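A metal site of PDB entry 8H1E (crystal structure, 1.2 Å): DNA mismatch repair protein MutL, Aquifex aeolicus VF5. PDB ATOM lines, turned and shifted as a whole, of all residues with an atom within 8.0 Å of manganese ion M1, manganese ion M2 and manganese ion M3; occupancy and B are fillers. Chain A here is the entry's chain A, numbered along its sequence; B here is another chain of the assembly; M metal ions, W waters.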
ATOM      1  N   ASP A  28      13.235  -2.982   7.754  1.00  0.00           N
ATOM      2  CA  ASP A  28      13.214  -1.691   8.437  1.00  0.00           C
ATOM      3  C   ASP A  28      14.640  -1.303   8.809  1.00  0.00           C
ATOM      4  O   ASP A  28      15.279  -1.988   9.618  1.00  0.00           O
ATOM      5  CB  ASP A  28      12.349  -1.816   9.708  1.00  0.00           C
ATOM      6  CG  ASP A  28      12.107  -0.500  10.405  1.00  0.00           C
ATOM      7  OD1 ASP A  28      13.084   0.188  10.753  1.00  0.00           O
ATOM      8  OD2 ASP A  28      10.931  -0.182  10.651  1.00  0.00           O
ATOM      9  N   HIS A  30      15.903   1.082  10.661  1.00  0.00           N
ATOM     10  CA  HIS A  30      16.140   1.369  12.075  1.00  0.00           C
ATOM     11  C   HIS A  30      16.179   0.084  12.882  1.00  0.00           C
ATOM     12  O   HIS A  30      17.098  -0.138  13.689  1.00  0.00           O
ATOM     13  CB  HIS A  30      15.082   2.289  12.649  1.00  0.00           C
ATOM     14  CG  HIS A  30      15.159   2.388  14.140  1.00  0.00           C
ATOM     15  ND1 HIS A  30      16.150   3.107  14.773  1.00  0.00           N
ATOM     16  CD2 HIS A  30      14.440   1.802  15.123  1.00  0.00           C
ATOM     17  CE1 HIS A  30      16.000   2.999  16.087  1.00  0.00           C
ATOM     18  NE2 HIS A  30      14.976   2.207  16.321  1.00  0.00           N
ATOM     19  N   LEU A  31      15.171  -0.781  12.695  1.00  0.00           N
ATOM     20  CA  LEU A  31      15.114  -2.009  13.480  1.00  0.00           C
ATOM     21  C   LEU A  31      16.304  -2.919  13.181  1.00  0.00           C
ATOM     22  O   LEU A  31      16.832  -3.574  14.095  1.00  0.00           O
ATOM     23  CB  LEU A  31      13.814  -2.759  13.197  1.00  0.00           C
ATOM     24  CG  LEU A  31      12.487  -2.131  13.640  1.00  0.00           C
ATOM     25  CD1 LEU A  31      11.321  -3.036  13.299  1.00  0.00           C
ATOM     26  CD2 LEU A  31      12.457  -1.784  15.109  1.00  0.00           C
ATOM     27  N   LEU A  32      16.766  -2.956  11.926  1.00  0.00           N
ATOM     28  CA  LEU A  32      17.941  -3.766  11.600  1.00  0.00           C
ATOM     29  C   LEU A  32      19.184  -3.230  12.291  1.00  0.00           C
ATOM     30  O   LEU A  32      19.906  -3.992  12.955  1.00  0.00           O
ATOM     31  CB  LEU A  32      18.141  -3.809  10.092  1.00  0.00           C
ATOM     32  CG  LEU A  32      19.440  -4.434   9.598  1.00  0.00           C
ATOM     33  CD1 LEU A  32      19.630  -5.845  10.174  1.00  0.00           C
ATOM     34  CD2 LEU A  32      19.527  -4.452   8.064  1.00  0.00           C
ATOM     35  N   GLU A  34      19.348  -1.353  14.878  1.00  0.00           N
ATOM     36  CA  GLU A  34      19.175  -1.524  16.314  1.00  0.00           C
ATOM     37  C   GLU A  34      19.512  -2.947  16.734  1.00  0.00           C
ATOM     38  O   GLU A  34      20.141  -3.161  17.769  1.00  0.00           O
ATOM     39  CB  GLU A  34      17.740  -1.187  16.720  1.00  0.00           C
ATOM     40  CG  GLU A  34      17.445  -1.238  18.214  1.00  0.00           C
ATOM     41  CD  GLU A  34      15.958  -1.066  18.514  1.00  0.00           C
ATOM     42  OE1 GLU A  34      15.158  -1.981  18.205  1.00  0.00           O
ATOM     43  OE2 GLU A  34      15.592   0.016  19.007  1.00  0.00           O
ATOM     44  N   ARG A  35      19.101  -3.920  15.925  1.00  0.00           N
ATOM     45  CA  ARG A  35      19.441  -5.317  16.210  1.00  0.00           C
ATOM     46  C   ARG A  35      20.947  -5.559  16.103  1.00  0.00           C
ATOM     47  O   ARG A  35      21.541  -6.209  16.976  1.00  0.00           O
ATOM     48  CB  ARG A  35      18.650  -6.253  15.305  1.00  0.00           C
ATOM     49  CG  ARG A  35      18.825  -7.731  15.633  1.00  0.00           C
ATOM     50  CD  ARG A  35      17.921  -8.110  16.800  1.00  0.00           C
ATOM     51  NE  ARG A  35      18.538  -9.072  17.699  1.00  0.00           N
ATOM     52  CZ  ARG A  35      17.936  -9.566  18.769  1.00  0.00           C
ATOM     53  NH1 ARG A  35      16.685  -9.256  19.072  1.00  0.00           N
ATOM     54  NH2 ARG A  35      18.607 -10.390  19.574  1.00  0.00           N
ATOM     55  N   GLU A  44      19.736  -2.318  25.012  1.00  0.00           N
ATOM     56  CA  GLU A  44      18.718  -1.968  24.019  1.00  0.00           C
ATOM     57  C   GLU A  44      18.493  -0.459  23.914  1.00  0.00           C
ATOM     58  O   GLU A  44      18.191   0.031  22.822  1.00  0.00           O
ATOM     59  CB  GLU A  44      17.410  -2.741  24.262  1.00  0.00           C
ATOM     60  CG  GLU A  44      16.400  -2.005  25.103  1.00  0.00           C
ATOM     61  CD  GLU A  44      15.100  -2.787  25.281  1.00  0.00           C
ATOM     62  OE1 GLU A  44      15.072  -3.987  24.928  1.00  0.00           O
ATOM     63  OE2 GLU A  44      14.129  -2.195  25.793  1.00  0.00           O
ATOM     64  N   ASN A  45      18.666   0.277  25.008  1.00  0.00           N
ATOM     65  CA  ASN A  45      18.488   1.725  24.950  1.00  0.00           C
ATOM     66  C   ASN A  45      19.610   2.362  24.143  1.00  0.00           C
ATOM     67  O   ASN A  45      19.372   3.251  23.311  1.00  0.00           O
ATOM     68  CB  ASN A  45      18.497   2.307  26.364  1.00  0.00           C
ATOM     69  CG  ASN A  45      17.190   2.105  27.079  1.00  0.00           C
ATOM     70  OD1 ASN A  45      16.218   1.632  26.503  1.00  0.00           O
ATOM     71  ND2 ASN A  45      17.145   2.487  28.357  1.00  0.00           N
ATOM     72  N   LEU A  46      20.841   1.913  24.374  1.00  0.00           N
ATOM     73  CA  LEU A  46      21.979   2.463  23.645  1.00  0.00           C
ATOM     74  C   LEU A  46      21.906   2.064  22.180  1.00  0.00           C
ATOM     75  O   LEU A  46      22.151   2.885  21.286  1.00  0.00           O
ATOM     76  CB  LEU A  46      23.283   1.949  24.265  1.00  0.00           C
ATOM     77  CG  LEU A  46      24.581   2.458  23.612  1.00  0.00           C
ATOM     78  CD1 LEU A  46      24.635   3.963  23.694  1.00  0.00           C
ATOM     79  CD2 LEU A  46      25.832   1.847  24.220  1.00  0.00           C
ATOM     80  N   ALA A  47      21.581   0.801  21.920  1.00  0.00           N
ATOM     81  CA  ALA A  47      21.459   0.347  20.536  1.00  0.00           C
ATOM     82  C   ALA A  47      20.424   1.173  19.780  1.00  0.00           C
ATOM     83  O   ALA A  47      20.649   1.558  18.631  1.00  0.00           O
ATOM     84  CB  ALA A  47      21.105  -1.142  20.503  1.00  0.00           C
ATOM     85  N   CYS A  48      19.302   1.478  20.421  1.00  0.00           N
ATOM     86  CA  CYS A  48      18.258   2.244  19.748  1.00  0.00           C
ATOM     87  C   CYS A  48      18.754   3.653  19.433  1.00  0.00           C
ATOM     88  O   CYS A  48      18.624   4.112  18.298  1.00  0.00           O
ATOM     89  CB  CYS A  48      17.013   2.307  20.624  1.00  0.00           C
ATOM     90  SG  CYS A  48      15.702   3.342  19.884  1.00  0.00           S
ATOM     91  N   ARG A  49      19.345   4.345  20.427  1.00  0.00           N
ATOM     92  CA  ARG A  49      19.605   5.775  20.285  1.00  0.00           C
ATOM     93  C   ARG A  49      20.726   6.067  19.279  1.00  0.00           C
ATOM     94  O   ARG A  49      20.761   7.170  18.699  1.00  0.00           O
ATOM     95  CB  ARG A  49      19.927   6.422  21.636  1.00  0.00           C
ATOM     96  CG  ARG A  49      21.325   6.119  22.186  1.00  0.00           C
ATOM     97  CD  ARG A  49      21.398   6.297  23.678  1.00  0.00           C
ATOM     98  NE  ARG A  49      21.108   7.658  24.100  1.00  0.00           N
ATOM     99  CZ  ARG A  49      20.978   8.037  25.369  1.00  0.00           C
ATOM    100  NH1 ARG A  49      21.081   7.162  26.364  1.00  0.00           N
ATOM    101  NH2 ARG A  49      20.762   9.322  25.647  1.00  0.00           N
ATOM    102  N   SER A  51      21.290   4.165  16.503  1.00  0.00           N
ATOM    103  CA  SER A  51      20.985   3.615  15.197  1.00  0.00           C
ATOM    104  C   SER A  51      20.347   4.646  14.273  1.00  0.00           C
ATOM    105  O   SER A  51      19.814   5.669  14.712  1.00  0.00           O
ATOM    106  CB  SER A  51      20.017   2.456  15.349  1.00  0.00           C
ATOM    107  OG  SER A  51      20.627   1.393  16.025  1.00  0.00           O
ATOM    108  N   VAL A  52      20.462   4.367  12.977  1.00  0.00           N
ATOM    109  CA  VAL A  52      19.809   5.189  11.979  1.00  0.00           C
ATOM    110  C   VAL A  52      18.307   5.214  12.244  1.00  0.00           C
ATOM    111  O   VAL A  52      17.717   4.271  12.776  1.00  0.00           O
ATOM    112  CB  VAL A  52      20.088   4.646  10.563  1.00  0.00           C
ATOM    113  CG1 VAL A  52      19.393   3.308  10.352  1.00  0.00           C
ATOM    114  CG2 VAL A  52      19.650   5.643   9.524  1.00  0.00           C
ATOM    115  N   LYS A  53      17.675   6.314  11.882  1.00  0.00           N
ATOM    116  CA  LYS A  53      16.232   6.451  11.995  1.00  0.00           C
ATOM    117  C   LYS A  53      15.575   6.351  10.632  1.00  0.00           C
ATOM    118  O   LYS A  53      16.205   6.547   9.592  1.00  0.00           O
ATOM    119  CB  LYS A  53      15.881   7.772  12.651  1.00  0.00           C
ATOM    120  CG  LYS A  53      16.407   7.847  14.070  1.00  0.00           C
ATOM    121  CD  LYS A  53      16.022   9.124  14.764  1.00  0.00           C
ATOM    122  CE  LYS A  53      16.770   9.256  16.079  1.00  0.00           C
ATOM    123  NZ  LYS A  53      16.555   8.109  16.993  1.00  0.00           N
ATOM    124  N   VAL A  78      13.459 -10.305  14.832  1.00  0.00           N
ATOM    125  CA  VAL A  78      12.791  -9.302  15.649  1.00  0.00           C
ATOM    126  C   VAL A  78      13.831  -8.426  16.325  1.00  0.00           C
ATOM    127  O   VAL A  78      14.932  -8.873  16.645  1.00  0.00           O
ATOM    128  CB  VAL A  78      11.873  -9.953  16.700  1.00  0.00           C
ATOM    129  CG1 VAL A  78      10.604 -10.493  16.040  1.00  0.00           C
ATOM    130  CG2 VAL A  78      12.617 -11.021  17.500  1.00  0.00           C
ATOM    131  N   CYS A  79      13.467  -7.167  16.553  1.00  0.00           N
ATOM    132  CA  CYS A  79      14.382  -6.265  17.250  1.00  0.00           C
ATOM    133  C   CYS A  79      14.318  -6.602  18.740  1.00  0.00           C
ATOM    134  O   CYS A  79      13.512  -7.446  19.163  1.00  0.00           O
ATOM    135  CB  CYS A  79      13.946  -4.804  17.052  1.00  0.00           C
ATOM    136  SG  CYS A  79      12.486  -4.268  17.983  1.00  0.00           S
ATOM    137  N   PRO A  80      15.177  -5.985  19.574  1.00  0.00           N
ATOM    138  CA  PRO A  80      15.131  -6.293  21.013  1.00  0.00           C
ATOM    139  C   PRO A  80      13.789  -6.025  21.681  1.00  0.00           C
ATOM    140  O   PRO A  80      13.521  -6.590  22.740  1.00  0.00           O
ATOM    141  CB  PRO A  80      16.219  -5.393  21.634  1.00  0.00           C
ATOM    142  CG  PRO A  80      16.805  -4.616  20.547  1.00  0.00           C
ATOM    143  CD  PRO A  80      16.346  -5.152  19.229  1.00  0.00           C
ATOM    144  N   HIS A  81      12.963  -5.148  21.118  1.00  0.00           N
ATOM    145  CA  HIS A  81      11.620  -4.898  21.626  1.00  0.00           C
ATOM    146  C   HIS A  81      10.582  -5.855  21.062  1.00  0.00           C
ATOM    147  O   HIS A  81       9.413  -5.757  21.434  1.00  0.00           O
ATOM    148  CB  HIS A  81      11.194  -3.459  21.335  1.00  0.00           C
ATOM    149  CG  HIS A  81      12.187  -2.449  21.809  1.00  0.00           C
ATOM    150  ND1 HIS A  81      13.135  -1.888  20.979  1.00  0.00           N
ATOM    151  CD2 HIS A  81      12.393  -1.911  23.035  1.00  0.00           C
ATOM    152  CE1 HIS A  81      13.873  -1.040  21.678  1.00  0.00           C
ATOM    153  NE2 HIS A  81      13.436  -1.031  22.927  1.00  0.00           N
ATOM    154  N   GLY A  82      10.978  -6.768  20.176  1.00  0.00           N
ATOM    155  CA  GLY A  82      10.082  -7.770  19.650  1.00  0.00           C
ATOM    156  C   GLY A  82       9.347  -7.380  18.389  1.00  0.00           C
ATOM    157  O   GLY A  82       8.475  -8.135  17.952  1.00  0.00           O
ATOM    158  N   ARG A  83       9.650  -6.220  17.793  1.00  0.00           N
ATOM    159  CA  ARG A  83       8.978  -5.880  16.537  1.00  0.00           C
ATOM    160  C   ARG A  83       9.640  -6.639  15.382  1.00  0.00           C
ATOM    161  O   ARG A  83      10.864  -6.732  15.329  1.00  0.00           O
ATOM    162  CB  ARG A  83       9.103  -4.380  16.244  1.00  0.00           C
ATOM    163  CG  ARG A  83       8.418  -3.470  17.262  1.00  0.00           C
ATOM    164  CD  ARG A  83       8.456  -2.027  16.771  1.00  0.00           C
ATOM    165  N   PRO A  84       8.863  -7.179  14.450  1.00  0.00           N
ATOM    166  CA  PRO A  84       9.455  -7.785  13.248  1.00  0.00           C
ATOM    167  C   PRO A  84      10.372  -6.805  12.526  1.00  0.00           C
ATOM    168  O   PRO A  84      10.000  -5.649  12.286  1.00  0.00           O
ATOM    169  CB  PRO A  84       8.237  -8.166  12.395  1.00  0.00           C
ATOM    170  CG  PRO A  84       7.123  -8.326  13.399  1.00  0.00           C
ATOM    171  CD  PRO A  84       7.391  -7.289  14.452  1.00  0.00           C
ATOM    172  N   ILE A  85      11.559  -7.278  12.165  1.00  0.00           N
ATOM    173  CA  ILE A  85      12.549  -6.438  11.495  1.00  0.00           C
ATOM    174  C   ILE A  85      12.150  -6.183  10.059  1.00  0.00           C
ATOM    175  O   ILE A  85      12.548  -5.175   9.470  1.00  0.00           O
ATOM    176  CB  ILE A  85      13.956  -7.055  11.629  1.00  0.00           C
ATOM    177  CG1 ILE A  85      14.441  -6.958  13.083  1.00  0.00           C
ATOM    178  CG2 ILE A  85      14.963  -6.428  10.644  1.00  0.00           C
ATOM    179  CD1 ILE A  85      15.740  -7.673  13.310  1.00  0.00           C
ATOM    180  N   VAL B  98       6.081  -3.923  10.829  1.00  0.00           N
ATOM    181  CA  VAL B  98       7.258  -3.513  11.590  1.00  0.00           C
ATOM    182  C   VAL B  98       6.881  -2.543  12.704  1.00  0.00           C
ATOM    183  O   VAL B  98       7.766  -1.935  13.334  1.00  0.00           O
ATOM    184  CB  VAL B  98       8.373  -2.962  10.665  1.00  0.00           C
ATOM    185  CG1 VAL B  98       8.812  -4.007   9.646  1.00  0.00           C
ATOM    186  CG2 VAL B  98       7.927  -1.671   9.950  1.00  0.00           C
ATOM    187  N   ARG B 100       4.994   0.338  12.543  1.00  0.00           N
ATOM    188  CA  ARG B 100       4.972   1.761  12.210  1.00  0.00           C
ATOM    189  C   ARG B 100       3.573   2.184  11.753  1.00  0.00           C
ATOM    190  O   ARG B 100       2.840   1.417  11.108  1.00  0.00           O
ATOM    191  CB  ARG B 100       5.943   2.089  11.071  1.00  0.00           C
ATOM    192  CG  ARG B 100       7.402   1.944  11.426  1.00  0.00           C
ATOM    193  CD  ARG B 100       8.310   2.376  10.281  1.00  0.00           C
ATOM    194  NE  ARG B 100       9.703   2.194  10.658  1.00  0.00           N
ATOM    195  CZ  ARG B 100      10.391   3.051  11.411  1.00  0.00           C
ATOM    196  NH1 ARG B 100       9.875   4.215  11.774  1.00  0.00           N
ATOM    197  NH2 ARG B 100      11.603   2.719  11.821  1.00  0.00           N
HETATM  198 MN    MN M   1      13.145  -1.997  18.743  1.00  0.00          MN
HETATM  199 MN    MN M   2      14.256   1.805  18.477  1.00  0.00          MN
HETATM  200 MN    MN M   3      13.935   3.661  21.701  1.00  0.00          MN
HETATM  201  O   HOH W   1      14.768   4.346  23.641  1.00  0.00           O
HETATM  202  O   HOH W   2      12.304   4.851  20.776  1.00  0.00           O
HETATM  203  O   HOH W   3      12.759   0.116  17.930  1.00  0.00           O
HETATM  204  O   HOH W   4      14.957   1.749  23.516  1.00  0.00           O
HETATM  205  O   HOH W   5      12.618   1.855  20.588  1.00  0.00           O
HETATM  206  O   HOH W   6      11.078  -1.115  18.666  1.00  0.00           O
HETATM  207  O   HOH W   7      12.760   3.418  18.074  1.00  0.00           O
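Leu 31 touches manganese ion M1. Four residues have an atom within 4 Å of manganese ion M1: Leu 31, Glu 34, Cys 79 and His 81. Along chain A the residues within 4 Å of manganese ion M1 span positions 31 to 81. The nearest printed residue that does not touch manganese ion M1 is Pro 80 (4.5 Å).
Water W4 bridges a ring nitrogen (NE2) of His 81 (3.2 Å) and the side-chain amide oxygen of Asn 45 (3.2 Å).
Manganese ion M1 is bound by OE1 of Glu 34, 2.1 Å away. Manganese ion M1 is bound by ND1 of His 81, at 2.2 Å. Water W6 binds manganese ion M1. Water W3 binds manganese ion M1, 2.3 Å away. SG of Cys 79 is bound to manganese ion M1 (2.5 Å). Manganese ion M1 has five donor atoms within binding distance.
The nearest printed residue that does not touch manganese ion M2 is His 81 (4.3 Å).
Manganese ion M3 is bound by water W1 (2.2 Å), water W2 (2.2 Å), water W5 (2.5 Å) and the side-chain sulfur of Cys 48 (2.6 Å). Slightly farther from manganese ion M3 lies water W4 (2.8 Å).
The backbone NH (N) of Glu 34 sits at hydrogen-bond distance from the side-chain hydroxyl (OG) of Ser 51. OE2 of Glu 44 is in hydrogen-bond range of NE2 of His 81 (3.2 Å). A ring nitrogen (ND1) of His 30 is in hydrogen-bond range of the backbone carbonyl oxygen (O) of Val 52, at 2.8 Å. The backbone NH of His 30 is in hydrogen-bond range of the side-chain carboxylate of Asp 28 (3.0 Å). N of Arg 83 sits close to SG of Cys 79 (3.4 Å). The side-chain sulfur (SG) of Cys 79 sits close to the backbone NH (N) of Gly 82 (3.7 Å). The backbone NH of Leu 31 lies within hydrogen-bond range of the side-chain carboxylate of Asp 28 (3.0 Å).
The nearest printed residue that does not touch manganese ion M3 is His 81 (4.7 Å).
Manganese ion M2 is bound by water W7, the side-chain carboxylate of Glu 34, a ring nitrogen (NE2) of His 30, water W3, the side-chain sulfur of Cys 48 and water W5. Manganese ion M2 has six donor atoms within binding distance.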
